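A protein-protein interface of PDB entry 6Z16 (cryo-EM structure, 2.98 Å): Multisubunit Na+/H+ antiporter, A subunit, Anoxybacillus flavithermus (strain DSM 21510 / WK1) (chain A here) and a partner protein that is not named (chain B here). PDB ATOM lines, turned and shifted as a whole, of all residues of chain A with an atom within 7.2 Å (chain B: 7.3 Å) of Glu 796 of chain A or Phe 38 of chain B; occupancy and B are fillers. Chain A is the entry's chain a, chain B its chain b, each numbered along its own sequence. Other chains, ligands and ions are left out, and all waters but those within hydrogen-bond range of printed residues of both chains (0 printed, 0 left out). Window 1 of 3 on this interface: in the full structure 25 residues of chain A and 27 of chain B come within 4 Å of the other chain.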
ATOM      1  N   THR A 701       1.201  26.448   8.033  1.00  0.00           N
ATOM      2  CA  THR A 701       0.862  25.749   9.266  1.00  0.00           C
ATOM      3  C   THR A 701       1.337  24.304   9.250  1.00  0.00           C
ATOM      4  O   THR A 701       1.762  23.791  10.289  1.00  0.00           O
ATOM      5  CB  THR A 701      -0.642  25.812   9.494  1.00  0.00           C
ATOM      6  OG1 THR A 701      -1.314  25.267   8.354  1.00  0.00           O
ATOM      7  CG2 THR A 701      -1.083  27.247   9.691  1.00  0.00           C
ATOM      8  N   VAL A 704       5.225  24.228  10.009  1.00  0.00           N
ATOM      9  CA  VAL A 704       5.574  24.502  11.406  1.00  0.00           C
ATOM     10  C   VAL A 704       5.097  23.382  12.328  1.00  0.00           C
ATOM     11  O   VAL A 704       5.847  22.916  13.203  1.00  0.00           O
ATOM     12  CB  VAL A 704       5.024  25.869  11.834  1.00  0.00           C
ATOM     13  CG1 VAL A 704       5.273  26.108  13.308  1.00  0.00           C
ATOM     14  CG2 VAL A 704       5.695  26.935  11.040  1.00  0.00           C
ATOM     15  N   ILE A 705       3.870  22.896  12.116  1.00  0.00           N
ATOM     16  CA  ILE A 705       3.312  21.860  12.973  1.00  0.00           C
ATOM     17  C   ILE A 705       4.037  20.530  12.794  1.00  0.00           C
ATOM     18  O   ILE A 705       4.278  19.819  13.779  1.00  0.00           O
ATOM     19  CB  ILE A 705       1.795  21.778  12.714  1.00  0.00           C
ATOM     20  CG1 ILE A 705       1.113  22.976  13.376  1.00  0.00           C
ATOM     21  CG2 ILE A 705       1.189  20.476  13.190  1.00  0.00           C
ATOM     22  CD1 ILE A 705      -0.307  23.172  12.986  1.00  0.00           C
ATOM     23  N   ASN A 782      -8.949  32.892   5.821  1.00  0.00           N
ATOM     24  CA  ASN A 782      -8.992  33.501   7.146  1.00  0.00           C
ATOM     25  C   ASN A 782     -10.364  34.100   7.442  1.00  0.00           C
ATOM     26  O   ASN A 782     -10.827  34.053   8.586  1.00  0.00           O
ATOM     27  CB  ASN A 782      -7.911  34.569   7.271  1.00  0.00           C
ATOM     28  CG  ASN A 782      -7.614  34.932   8.713  1.00  0.00           C
ATOM     29  OD1 ASN A 782      -8.139  34.321   9.638  1.00  0.00           O
ATOM     30  ND2 ASN A 782      -6.784  35.941   8.909  1.00  0.00           N
ATOM     31  N   LEU A 785     -12.425  31.480   8.497  1.00  0.00           N
ATOM     32  CA  LEU A 785     -12.025  31.006   9.819  1.00  0.00           C
ATOM     33  C   LEU A 785     -12.470  31.923  10.950  1.00  0.00           C
ATOM     34  O   LEU A 785     -12.630  31.452  12.081  1.00  0.00           O
ATOM     35  CB  LEU A 785     -10.516  30.828   9.898  1.00  0.00           C
ATOM     36  CG  LEU A 785      -9.879  29.620   9.233  1.00  0.00           C
ATOM     37  CD1 LEU A 785      -8.399  29.823   9.276  1.00  0.00           C
ATOM     38  CD2 LEU A 785     -10.259  28.352   9.957  1.00  0.00           C
ATOM     39  N   VAL A 786     -12.645  33.219  10.706  1.00  0.00           N
ATOM     40  CA  VAL A 786     -12.961  34.136  11.795  1.00  0.00           C
ATOM     41  C   VAL A 786     -14.297  34.840  11.634  1.00  0.00           C
ATOM     42  O   VAL A 786     -14.826  35.354  12.632  1.00  0.00           O
ATOM     43  CB  VAL A 786     -11.846  35.184  12.010  1.00  0.00           C
ATOM     44  CG1 VAL A 786     -10.516  34.520  12.261  1.00  0.00           C
ATOM     45  CG2 VAL A 786     -11.777  36.169  10.859  1.00  0.00           C
ATOM     46  N   PHE A 791     -17.408  30.451  14.763  1.00  0.00           N
ATOM     47  CA  PHE A 791     -17.949  29.856  15.973  1.00  0.00           C
ATOM     48  C   PHE A 791     -17.207  28.580  16.340  1.00  0.00           C
ATOM     49  O   PHE A 791     -17.091  28.257  17.524  1.00  0.00           O
ATOM     50  CB  PHE A 791     -19.446  29.602  15.793  1.00  0.00           C
ATOM     51  CG  PHE A 791     -20.123  29.062  17.015  1.00  0.00           C
ATOM     52  CD1 PHE A 791     -20.315  29.865  18.125  1.00  0.00           C
ATOM     53  CD2 PHE A 791     -20.595  27.763  17.045  1.00  0.00           C
ATOM     54  CE1 PHE A 791     -20.941  29.373  19.251  1.00  0.00           C
ATOM     55  CE2 PHE A 791     -21.223  27.266  18.166  1.00  0.00           C
ATOM     56  CZ  PHE A 791     -21.394  28.074  19.270  1.00  0.00           C
ATOM     57  N   ASP A 792     -16.674  27.864  15.354  1.00  0.00           N
ATOM     58  CA  ASP A 792     -15.910  26.652  15.616  1.00  0.00           C
ATOM     59  C   ASP A 792     -14.419  26.902  15.792  1.00  0.00           C
ATOM     60  O   ASP A 792     -13.705  25.993  16.224  1.00  0.00           O
ATOM     61  CB  ASP A 792     -16.147  25.630  14.501  1.00  0.00           C
ATOM     62  CG  ASP A 792     -15.902  26.197  13.122  1.00  0.00           C
ATOM     63  OD1 ASP A 792     -15.633  27.409  13.008  1.00  0.00           O
ATOM     64  OD2 ASP A 792     -15.990  25.426  12.143  1.00  0.00           O
ATOM     65  N   THR A 793     -13.931  28.099  15.468  1.00  0.00           N
ATOM     66  CA  THR A 793     -12.541  28.439  15.744  1.00  0.00           C
ATOM     67  C   THR A 793     -12.324  28.673  17.235  1.00  0.00           C
ATOM     68  O   THR A 793     -11.254  28.359  17.771  1.00  0.00           O
ATOM     69  CB  THR A 793     -12.152  29.667  14.919  1.00  0.00           C
ATOM     70  OG1 THR A 793     -12.440  29.414  13.540  1.00  0.00           O
ATOM     71  CG2 THR A 793     -10.674  29.983  15.043  1.00  0.00           C
ATOM     72  N   LEU A 794     -13.347  29.186  17.922  1.00  0.00           N
ATOM     73  CA  LEU A 794     -13.279  29.372  19.368  1.00  0.00           C
ATOM     74  C   LEU A 794     -13.066  28.049  20.094  1.00  0.00           C
ATOM     75  O   LEU A 794     -12.294  27.968  21.058  1.00  0.00           O
ATOM     76  CB  LEU A 794     -14.556  30.063  19.839  1.00  0.00           C
ATOM     77  CG  LEU A 794     -14.762  30.296  21.328  1.00  0.00           C
ATOM     78  CD1 LEU A 794     -13.638  31.116  21.918  1.00  0.00           C
ATOM     79  CD2 LEU A 794     -16.091  30.995  21.512  1.00  0.00           C
ATOM     80  N   PHE A 795     -13.653  26.977  19.585  1.00  0.00           N
ATOM     81  CA  PHE A 795     -13.521  25.714  20.283  1.00  0.00           C
ATOM     82  C   PHE A 795     -12.291  24.916  19.868  1.00  0.00           C
ATOM     83  O   PHE A 795     -11.853  24.064  20.639  1.00  0.00           O
ATOM     84  CB  PHE A 795     -14.807  24.909  20.120  1.00  0.00           C
ATOM     85  CG  PHE A 795     -15.993  25.593  20.724  1.00  0.00           C
ATOM     86  CD1 PHE A 795     -16.177  25.600  22.093  1.00  0.00           C
ATOM     87  CD2 PHE A 795     -16.899  26.260  19.928  1.00  0.00           C
ATOM     88  CE1 PHE A 795     -17.254  26.253  22.652  1.00  0.00           C
ATOM     89  CE2 PHE A 795     -17.980  26.915  20.480  1.00  0.00           C
ATOM     90  CZ  PHE A 795     -18.155  26.909  21.842  1.00  0.00           C
ATOM     91  N   GLU A 796     -11.665  25.208  18.727  1.00  0.00           N
ATOM     92  CA  GLU A 796     -10.341  24.633  18.505  1.00  0.00           C
ATOM     93  C   GLU A 796      -9.279  25.367  19.319  1.00  0.00           C
ATOM     94  O   GLU A 796      -8.284  24.747  19.731  1.00  0.00           O
ATOM     95  CB  GLU A 796      -9.985  24.627  17.017  1.00  0.00           C
ATOM     96  CG  GLU A 796      -9.710  25.984  16.424  1.00  0.00           C
ATOM     97  CD  GLU A 796      -9.515  25.955  14.957  1.00  0.00           C
ATOM     98  OE1 GLU A 796      -9.556  24.854  14.424  1.00  0.00           O
ATOM     99  OE2 GLU A 796      -9.348  27.018  14.332  1.00  0.00           O
ATOM    100  N   ILE A 797      -9.493  26.665  19.586  1.00  0.00           N
ATOM    101  CA  ILE A 797      -8.717  27.363  20.610  1.00  0.00           C
ATOM    102  C   ILE A 797      -8.886  26.668  21.956  1.00  0.00           C
ATOM    103  O   ILE A 797      -7.913  26.454  22.695  1.00  0.00           O
ATOM    104  CB  ILE A 797      -9.153  28.838  20.686  1.00  0.00           C
ATOM    105  CG1 ILE A 797      -8.830  29.596  19.415  1.00  0.00           C
ATOM    106  CG2 ILE A 797      -8.475  29.551  21.796  1.00  0.00           C
ATOM    107  CD1 ILE A 797      -9.616  30.871  19.353  1.00  0.00           C
ATOM    108  N   CYS A 798     -10.126  26.274  22.270  1.00  0.00           N
ATOM    109  CA  CYS A 798     -10.391  25.519  23.493  1.00  0.00           C
ATOM    110  C   CYS A 798      -9.687  24.164  23.505  1.00  0.00           C
ATOM    111  O   CYS A 798      -9.186  23.743  24.550  1.00  0.00           O
ATOM    112  CB  CYS A 798     -11.894  25.331  23.679  1.00  0.00           C
ATOM    113  SG  CYS A 798     -12.782  26.843  24.020  1.00  0.00           S
ATOM    114  N   VAL A 799      -9.648  23.468  22.360  1.00  0.00           N
ATOM    115  CA  VAL A 799      -8.977  22.166  22.271  1.00  0.00           C
ATOM    116  C   VAL A 799      -7.487  22.306  22.552  1.00  0.00           C
ATOM    117  O   VAL A 799      -6.908  21.525  23.321  1.00  0.00           O
ATOM    118  CB  VAL A 799      -9.232  21.517  20.895  1.00  0.00           C
ATOM    119  CG1 VAL A 799      -8.337  20.313  20.685  1.00  0.00           C
ATOM    120  CG2 VAL A 799     -10.661  21.061  20.781  1.00  0.00           C
ATOM    121  N   LEU A 800      -6.854  23.329  21.966  1.00  0.00           N
ATOM    122  CA  LEU A 800      -5.437  23.574  22.225  1.00  0.00           C
ATOM    123  C   LEU A 800      -5.186  23.955  23.681  1.00  0.00           C
ATOM    124  O   LEU A 800      -4.177  23.544  24.274  1.00  0.00           O
ATOM    125  CB  LEU A 800      -4.918  24.661  21.288  1.00  0.00           C
ATOM    126  CG  LEU A 800      -4.881  24.315  19.803  1.00  0.00           C
ATOM    127  CD1 LEU A 800      -4.472  25.526  19.000  1.00  0.00           C
ATOM    128  CD2 LEU A 800      -3.926  23.168  19.562  1.00  0.00           C
ATOM    129  N   ALA A 801      -6.113  24.710  24.283  1.00  0.00           N
ATOM    130  CA  ALA A 801      -5.972  25.086  25.688  1.00  0.00           C
ATOM    131  C   ALA A 801      -6.070  23.874  26.611  1.00  0.00           C
ATOM    132  O   ALA A 801      -5.261  23.734  27.542  1.00  0.00           O
ATOM    133  CB  ALA A 801      -7.030  26.121  26.056  1.00  0.00           C
ATOM    134  N   ILE A 802      -7.048  22.992  26.359  1.00  0.00           N
ATOM    135  CA  ILE A 802      -7.200  21.761  27.138  1.00  0.00           C
ATOM    136  C   ILE A 802      -5.976  20.871  26.973  1.00  0.00           C
ATOM    137  O   ILE A 802      -5.505  20.261  27.939  1.00  0.00           O
ATOM    138  CB  ILE A 802      -8.491  21.020  26.734  1.00  0.00           C
ATOM    139  CG1 ILE A 802      -9.726  21.848  27.040  1.00  0.00           C
ATOM    140  CG2 ILE A 802      -8.654  19.727  27.505  1.00  0.00           C
ATOM    141  CD1 ILE A 802     -10.942  21.372  26.284  1.00  0.00           C
ATOM    142  N   PHE B  27       0.903  38.261  11.187  1.00  0.00           N
ATOM    143  CA  PHE B  27      -0.326  38.438  11.948  1.00  0.00           C
ATOM    144  C   PHE B  27      -1.159  39.613  11.443  1.00  0.00           C
ATOM    145  O   PHE B  27      -2.378  39.485  11.292  1.00  0.00           O
ATOM    146  CB  PHE B  27      -0.004  38.605  13.426  1.00  0.00           C
ATOM    147  CG  PHE B  27      -1.198  38.907  14.255  1.00  0.00           C
ATOM    148  CD1 PHE B  27      -2.171  37.950  14.453  1.00  0.00           C
ATOM    149  CD2 PHE B  27      -1.345  40.145  14.848  1.00  0.00           C
ATOM    150  CE1 PHE B  27      -3.282  38.230  15.212  1.00  0.00           C
ATOM    151  CE2 PHE B  27      -2.450  40.431  15.610  1.00  0.00           C
ATOM    152  CZ  PHE B  27      -3.420  39.472  15.792  1.00  0.00           C
ATOM    153  N   GLY B  35      -1.556  34.091   5.923  1.00  0.00           N
ATOM    154  CA  GLY B  35      -1.139  34.331   7.286  1.00  0.00           C
ATOM    155  C   GLY B  35      -2.337  34.456   8.206  1.00  0.00           C
ATOM    156  O   GLY B  35      -3.489  34.343   7.793  1.00  0.00           O
ATOM    157  N   GLY B  36      -2.042  34.700   9.475  1.00  0.00           N
ATOM    158  CA  GLY B  36      -3.102  34.879  10.449  1.00  0.00           C
ATOM    159  C   GLY B  36      -2.562  34.720  11.859  1.00  0.00           C
ATOM    160  O   GLY B  36      -1.358  34.786  12.085  1.00  0.00           O
ATOM    161  N   GLY B  37      -3.491  34.506  12.792  1.00  0.00           N
ATOM    162  CA  GLY B  37      -3.108  34.345  14.182  1.00  0.00           C
ATOM    163  C   GLY B  37      -2.371  33.052  14.462  1.00  0.00           C
ATOM    164  O   GLY B  37      -1.503  33.013  15.340  1.00  0.00           O
ATOM    165  N   PHE B  38      -2.685  31.993  13.708  1.00  0.00           N
ATOM    166  CA  PHE B  38      -2.085  30.680  13.938  1.00  0.00           C
ATOM    167  C   PHE B  38      -0.593  30.692  13.645  1.00  0.00           C
ATOM    168  O   PHE B  38       0.229  30.423  14.529  1.00  0.00           O
ATOM    169  CB  PHE B  38      -2.781  29.631  13.071  1.00  0.00           C
ATOM    170  CG  PHE B  38      -4.203  29.381  13.449  1.00  0.00           C
ATOM    171  CD1 PHE B  38      -4.515  28.518  14.486  1.00  0.00           C
ATOM    172  CD2 PHE B  38      -5.231  30.015  12.772  1.00  0.00           C
ATOM    173  CE1 PHE B  38      -5.826  28.291  14.839  1.00  0.00           C
ATOM    174  CE2 PHE B  38      -6.545  29.792  13.121  1.00  0.00           C
ATOM    175  CZ  PHE B  38      -6.841  28.930  14.157  1.00  0.00           C
ATOM    176  N   ILE B  39      -0.227  31.025  12.405  1.00  0.00           N
ATOM    177  CA  ILE B  39       1.169  30.992  11.991  1.00  0.00           C
ATOM    178  C   ILE B  39       1.974  32.097  12.674  1.00  0.00           C
ATOM    179  O   ILE B  39       3.149  31.895  13.018  1.00  0.00           O
ATOM    180  CB  ILE B  39       1.244  31.045  10.450  1.00  0.00           C
ATOM    181  CG1 ILE B  39       2.670  30.814   9.964  1.00  0.00           C
ATOM    182  CG2 ILE B  39       0.622  32.312   9.879  1.00  0.00           C
ATOM    183  CD1 ILE B  39       3.154  29.445  10.255  1.00  0.00           C
ATOM    184  N   GLY B  40       1.343  33.241  12.954  1.00  0.00           N
ATOM    185  CA  GLY B  40       2.034  34.306  13.656  1.00  0.00           C
ATOM    186  C   GLY B  40       2.333  33.947  15.096  1.00  0.00           C
ATOM    187  O   GLY B  40       3.430  34.220  15.597  1.00  0.00           O
ATOM    188  N   GLY B  41       1.380  33.304  15.772  1.00  0.00           N
ATOM    189  CA  GLY B  41       1.629  32.854  17.127  1.00  0.00           C
ATOM    190  C   GLY B  41       2.653  31.741  17.185  1.00  0.00           C
ATOM    191  O   GLY B  41       3.495  31.707  18.091  1.00  0.00           O
ATOM    192  N   LEU B  42       2.620  30.841  16.195  1.00  0.00           N
ATOM    193  CA  LEU B  42       3.597  29.759  16.131  1.00  0.00           C
ATOM    194  C   LEU B  42       5.007  30.285  15.906  1.00  0.00           C
ATOM    195  O   LEU B  42       5.961  29.779  16.502  1.00  0.00           O
ATOM    196  CB  LEU B  42       3.217  28.758  15.041  1.00  0.00           C
ATOM    197  CG  LEU B  42       2.047  27.823  15.351  1.00  0.00           C
ATOM    198  CD1 LEU B  42       1.643  27.010  14.135  1.00  0.00           C
ATOM    199  CD2 LEU B  42       2.416  26.920  16.507  1.00  0.00           C
ATOM    200  N   MET B  43       5.167  31.337  15.104  1.00  0.00           N
ATOM    201  CA  MET B  43       6.530  31.811  14.908  1.00  0.00           C
ATOM    202  C   MET B  43       7.002  32.803  15.961  1.00  0.00           C
ATOM    203  O   MET B  43       8.217  32.920  16.167  1.00  0.00           O
ATOM    204  CB  MET B  43       6.721  32.395  13.509  1.00  0.00           C
ATOM    205  CG  MET B  43       6.537  31.342  12.432  1.00  0.00           C
ATOM    206  SD  MET B  43       7.256  29.734  12.873  1.00  0.00           S
ATOM    207  CE  MET B  43       9.027  29.996  12.986  1.00  0.00           C
ATOM    208  N   THR B  44       6.093  33.494  16.653  1.00  0.00           N
ATOM    209  CA  THR B  44       6.494  34.198  17.867  1.00  0.00           C
ATOM    210  C   THR B  44       7.001  33.212  18.911  1.00  0.00           C
ATOM    211  O   THR B  44       8.053  33.429  19.542  1.00  0.00           O
ATOM    212  CB  THR B  44       5.320  35.005  18.412  1.00  0.00           C
ATOM    213  OG1 THR B  44       4.894  35.951  17.427  1.00  0.00           O
ATOM    214  CG2 THR B  44       5.718  35.749  19.674  1.00  0.00           C
ATOM    215  N   LEU B  76      -8.546  33.494  25.244  1.00  0.00           N
ATOM    216  CA  LEU B  76      -9.912  32.973  25.305  1.00  0.00           C
ATOM    217  C   LEU B  76     -10.911  34.058  25.700  1.00  0.00           C
ATOM    218  O   LEU B  76     -11.996  34.158  25.106  1.00  0.00           O
ATOM    219  CB  LEU B  76      -9.954  31.807  26.289  1.00  0.00           C
ATOM    220  CG  LEU B  76      -9.352  30.486  25.819  1.00  0.00           C
ATOM    221  CD1 LEU B  76      -9.054  29.568  26.982  1.00  0.00           C
ATOM    222  CD2 LEU B  76     -10.361  29.833  24.917  1.00  0.00           C
ATOM    223  N   PHE B 117     -10.369  38.938  17.422  1.00  0.00           N
ATOM    224  CA  PHE B 117     -10.570  37.496  17.492  1.00  0.00           C
ATOM    225  C   PHE B 117      -9.291  36.761  17.093  1.00  0.00           C
ATOM    226  O   PHE B 117      -8.846  35.834  17.789  1.00  0.00           O
ATOM    227  CB  PHE B 117     -11.744  37.110  16.594  1.00  0.00           C
ATOM    228  CG  PHE B 117     -12.150  35.680  16.704  1.00  0.00           C
ATOM    229  CD1 PHE B 117     -12.889  35.240  17.786  1.00  0.00           C
ATOM    230  CD2 PHE B 117     -11.802  34.774  15.723  1.00  0.00           C
ATOM    231  CE1 PHE B 117     -13.268  33.921  17.889  1.00  0.00           C
ATOM    232  CE2 PHE B 117     -12.175  33.453  15.821  1.00  0.00           C
ATOM    233  CZ  PHE B 117     -12.909  33.027  16.906  1.00  0.00           C
ATOM    234  N   ASP B 118      -8.657  37.213  16.000  1.00  0.00           N
ATOM    235  CA  ASP B 118      -7.317  36.750  15.637  1.00  0.00           C
ATOM    236  C   ASP B 118      -6.286  37.010  16.726  1.00  0.00           C
ATOM    237  O   ASP B 118      -5.342  36.232  16.877  1.00  0.00           O
ATOM    238  CB  ASP B 118      -6.853  37.418  14.344  1.00  0.00           C
ATOM    239  CG  ASP B 118      -7.382  36.734  13.112  1.00  0.00           C
ATOM    240  OD1 ASP B 118      -7.539  35.500  13.158  1.00  0.00           O
ATOM    241  OD2 ASP B 118      -7.621  37.418  12.091  1.00  0.00           O
ATOM    242  N   VAL B 121      -6.648  34.319  19.204  1.00  0.00           N
ATOM    243  CA  VAL B 121      -6.010  33.142  18.601  1.00  0.00           C
ATOM    244  C   VAL B 121      -4.496  33.198  18.781  1.00  0.00           C
ATOM    245  O   VAL B 121      -3.860  32.215  19.180  1.00  0.00           O
ATOM    246  CB  VAL B 121      -6.372  33.035  17.107  1.00  0.00           C
ATOM    247  CG1 VAL B 121      -5.654  31.872  16.467  1.00  0.00           C
ATOM    248  CG2 VAL B 121      -7.850  32.892  16.893  1.00  0.00           C
ATOM    249  N   TYR B 122      -3.920  34.374  18.518  1.00  0.00           N
ATOM    250  CA  TYR B 122      -2.482  34.607  18.613  1.00  0.00           C
ATOM    251  C   TYR B 122      -1.964  34.345  20.021  1.00  0.00           C
ATOM    252  O   TYR B 122      -0.973  33.621  20.205  1.00  0.00           O
ATOM    253  CB  TYR B 122      -2.197  36.050  18.193  1.00  0.00           C
ATOM    254  CG  TYR B 122      -0.747  36.460  18.189  1.00  0.00           C
ATOM    255  CD1 TYR B 122       0.067  36.194  17.101  1.00  0.00           C
ATOM    256  CD2 TYR B 122      -0.189  37.107  19.284  1.00  0.00           C
ATOM    257  CE1 TYR B 122       1.394  36.568  17.102  1.00  0.00           C
ATOM    258  CE2 TYR B 122       1.134  37.473  19.298  1.00  0.00           C
ATOM    259  CZ  TYR B 122       1.921  37.204  18.205  1.00  0.00           C
ATOM    260  OH  TYR B 122       3.241  37.580  18.214  1.00  0.00           O
ATOM    261  N   VAL B 124      -3.370  32.619  22.479  1.00  0.00           N
ATOM    262  CA  VAL B 124      -3.514  31.237  22.933  1.00  0.00           C
ATOM    263  C   VAL B 124      -2.487  30.332  22.253  1.00  0.00           C
ATOM    264  O   VAL B 124      -1.929  29.439  22.893  1.00  0.00           O
ATOM    265  CB  VAL B 124      -4.956  30.741  22.729  1.00  0.00           C
ATOM    266  CG1 VAL B 124      -5.090  29.288  23.144  1.00  0.00           C
ATOM    267  CG2 VAL B 124      -5.891  31.563  23.565  1.00  0.00           C
ATOM    268  N   VAL B 125      -2.170  30.586  20.978  1.00  0.00           N
ATOM    269  CA  VAL B 125      -1.173  29.764  20.290  1.00  0.00           C
ATOM    270  C   VAL B 125       0.216  29.962  20.896  1.00  0.00           C
ATOM    271  O   VAL B 125       0.927  28.977  21.166  1.00  0.00           O
ATOM    272  CB  VAL B 125      -1.190  30.047  18.776  1.00  0.00           C
ATOM    273  CG1 VAL B 125      -0.008  29.409  18.099  1.00  0.00           C
ATOM    274  CG2 VAL B 125      -2.443  29.478  18.164  1.00  0.00           C
ATOM    275  N   VAL B 126       0.591  31.222  21.179  1.00  0.00           N
ATOM    276  CA  VAL B 126       1.867  31.507  21.848  1.00  0.00           C
ATOM    277  C   VAL B 126       1.925  30.831  23.213  1.00  0.00           C
ATOM    278  O   VAL B 126       2.903  30.140  23.544  1.00  0.00           O
ATOM    279  CB  VAL B 126       2.087  33.025  21.979  1.00  0.00           C
ATOM    280  CG1 VAL B 126       3.302  33.310  22.833  1.00  0.00           C
ATOM    281  CG2 VAL B 126       2.284  33.648  20.638  1.00  0.00           C
ATOM    282  N   THR B 129       1.990  26.756  22.965  1.00  0.00           N
ATOM    283  CA  THR B 129       3.279  26.251  22.502  1.00  0.00           C
ATOM    284  C   THR B 129       4.359  26.426  23.563  1.00  0.00           C
ATOM    285  O   THR B 129       5.142  25.498  23.827  1.00  0.00           O
ATOM    286  CB  THR B 129       3.675  26.958  21.210  1.00  0.00           C
ATOM    287  OG1 THR B 129       2.632  26.796  20.246  1.00  0.00           O
ATOM    288  CG2 THR B 129       4.923  26.349  20.646  1.00  0.00           C
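Hydrophobic or aromatic side chains of chain B within 4 Å of the printed part of chain A: Phe 38, Ile 39, Leu 42, Met 43, Leu 76, Phe 117, Val 121 and Val 124.
Of the 18 printed residues of chain A, 8 touch a printed residue of chain B.
Printed residues of chain A that touch a printed residue of chain B: Val 704, Asn 782, Val 786, Thr 793, Leu 794, Glu 796, Ile 797 and Cys 798.
Hydrophobic or aromatic side chains of chain A that line the printed part of chain B: Val 704, Val 786 and Ile 797.
Among the printed residues, no Asp or Glu carboxylate lies within 4 Å of a Lys or Arg side-chain nitrogen of the other chain.
The side-chain hydroxyl (OG1) of Thr 793 of chain A lies within hydrogen-bond range of the backbone carbonyl oxygen (O) of Leu 785 of chain A, 2.5 Å away.
SG of Cys 798 of chain A is in hydrogen-bond range of O of Leu 794 of chain A.
Among the printed residues, merely in contact across the chains: Val 704 of chain A with Ile 39 of chain B (3.7 Å), Val 704 of chain A with Leu 42 of chain B (3.8 Å), Val 704 of chain A with Met 43 of chain B (3.7 Å), Asn 782 of chain A with Gly 35 of chain B (3.8 Å), Asn 782 of chain A with Asp 118 of chain B (3.6 Å), Val 786 of chain A with Phe 117 of chain B (3.7 Å), Val 786 of chain A with Asp 118 of chain B (3.3 Å), Thr 793 of chain A with Phe 117 of chain B (3.9 Å), Leu 794 of chain A with Phe 117 of chain B (3.997 Å), Glu 796 of chain A with Phe 38 of chain B (3.2 Å), Ile 797 of chain A with Leu 76 of chain B (3.7 Å), Ile 797 of chain A with Val 121 of chain B (3.6 Å), Ile 797 of chain A with Val 124 of chain B (3.7 Å) and Cys 798 of chain A with Leu 76 of chain B (3.95 Å).
Of the printed residues of chain B, Val 786 of chain A touches Phe 117 and Asp 118.
Printed residues of chain B within 4 Å of Leu 794 of chain A: Phe 117 (3.997 Å).
Gly 37 of chain B touches none of the printed residues of chain A.
Of chain A, only Glu 796 comes within 4 Å of Phe 38 of chain B.
Of the printed residues of chain A, Ile 39 of chain B touches Val 704.
Printed residues of chain A within 4 Å of Met 43 of chain B: Val 704 (3.7 Å).
Printed residues of chain A within 4 Å of Asp 118 of chain B: Asn 782 (3.6 Å) and Val 786 (3.3 Å).
The nearest residue of chain B that does not touch Glu 796 of chain A is Val 121 of chain B (6.5 Å).
The nearest residue of chain A that does not touch Phe 38 of chain B is Thr 793 of chain A (4.1 Å).
The nearest printed residue of chain A that does not touch Phe 117 of chain B is Leu 785 of chain A (4.3 Å).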
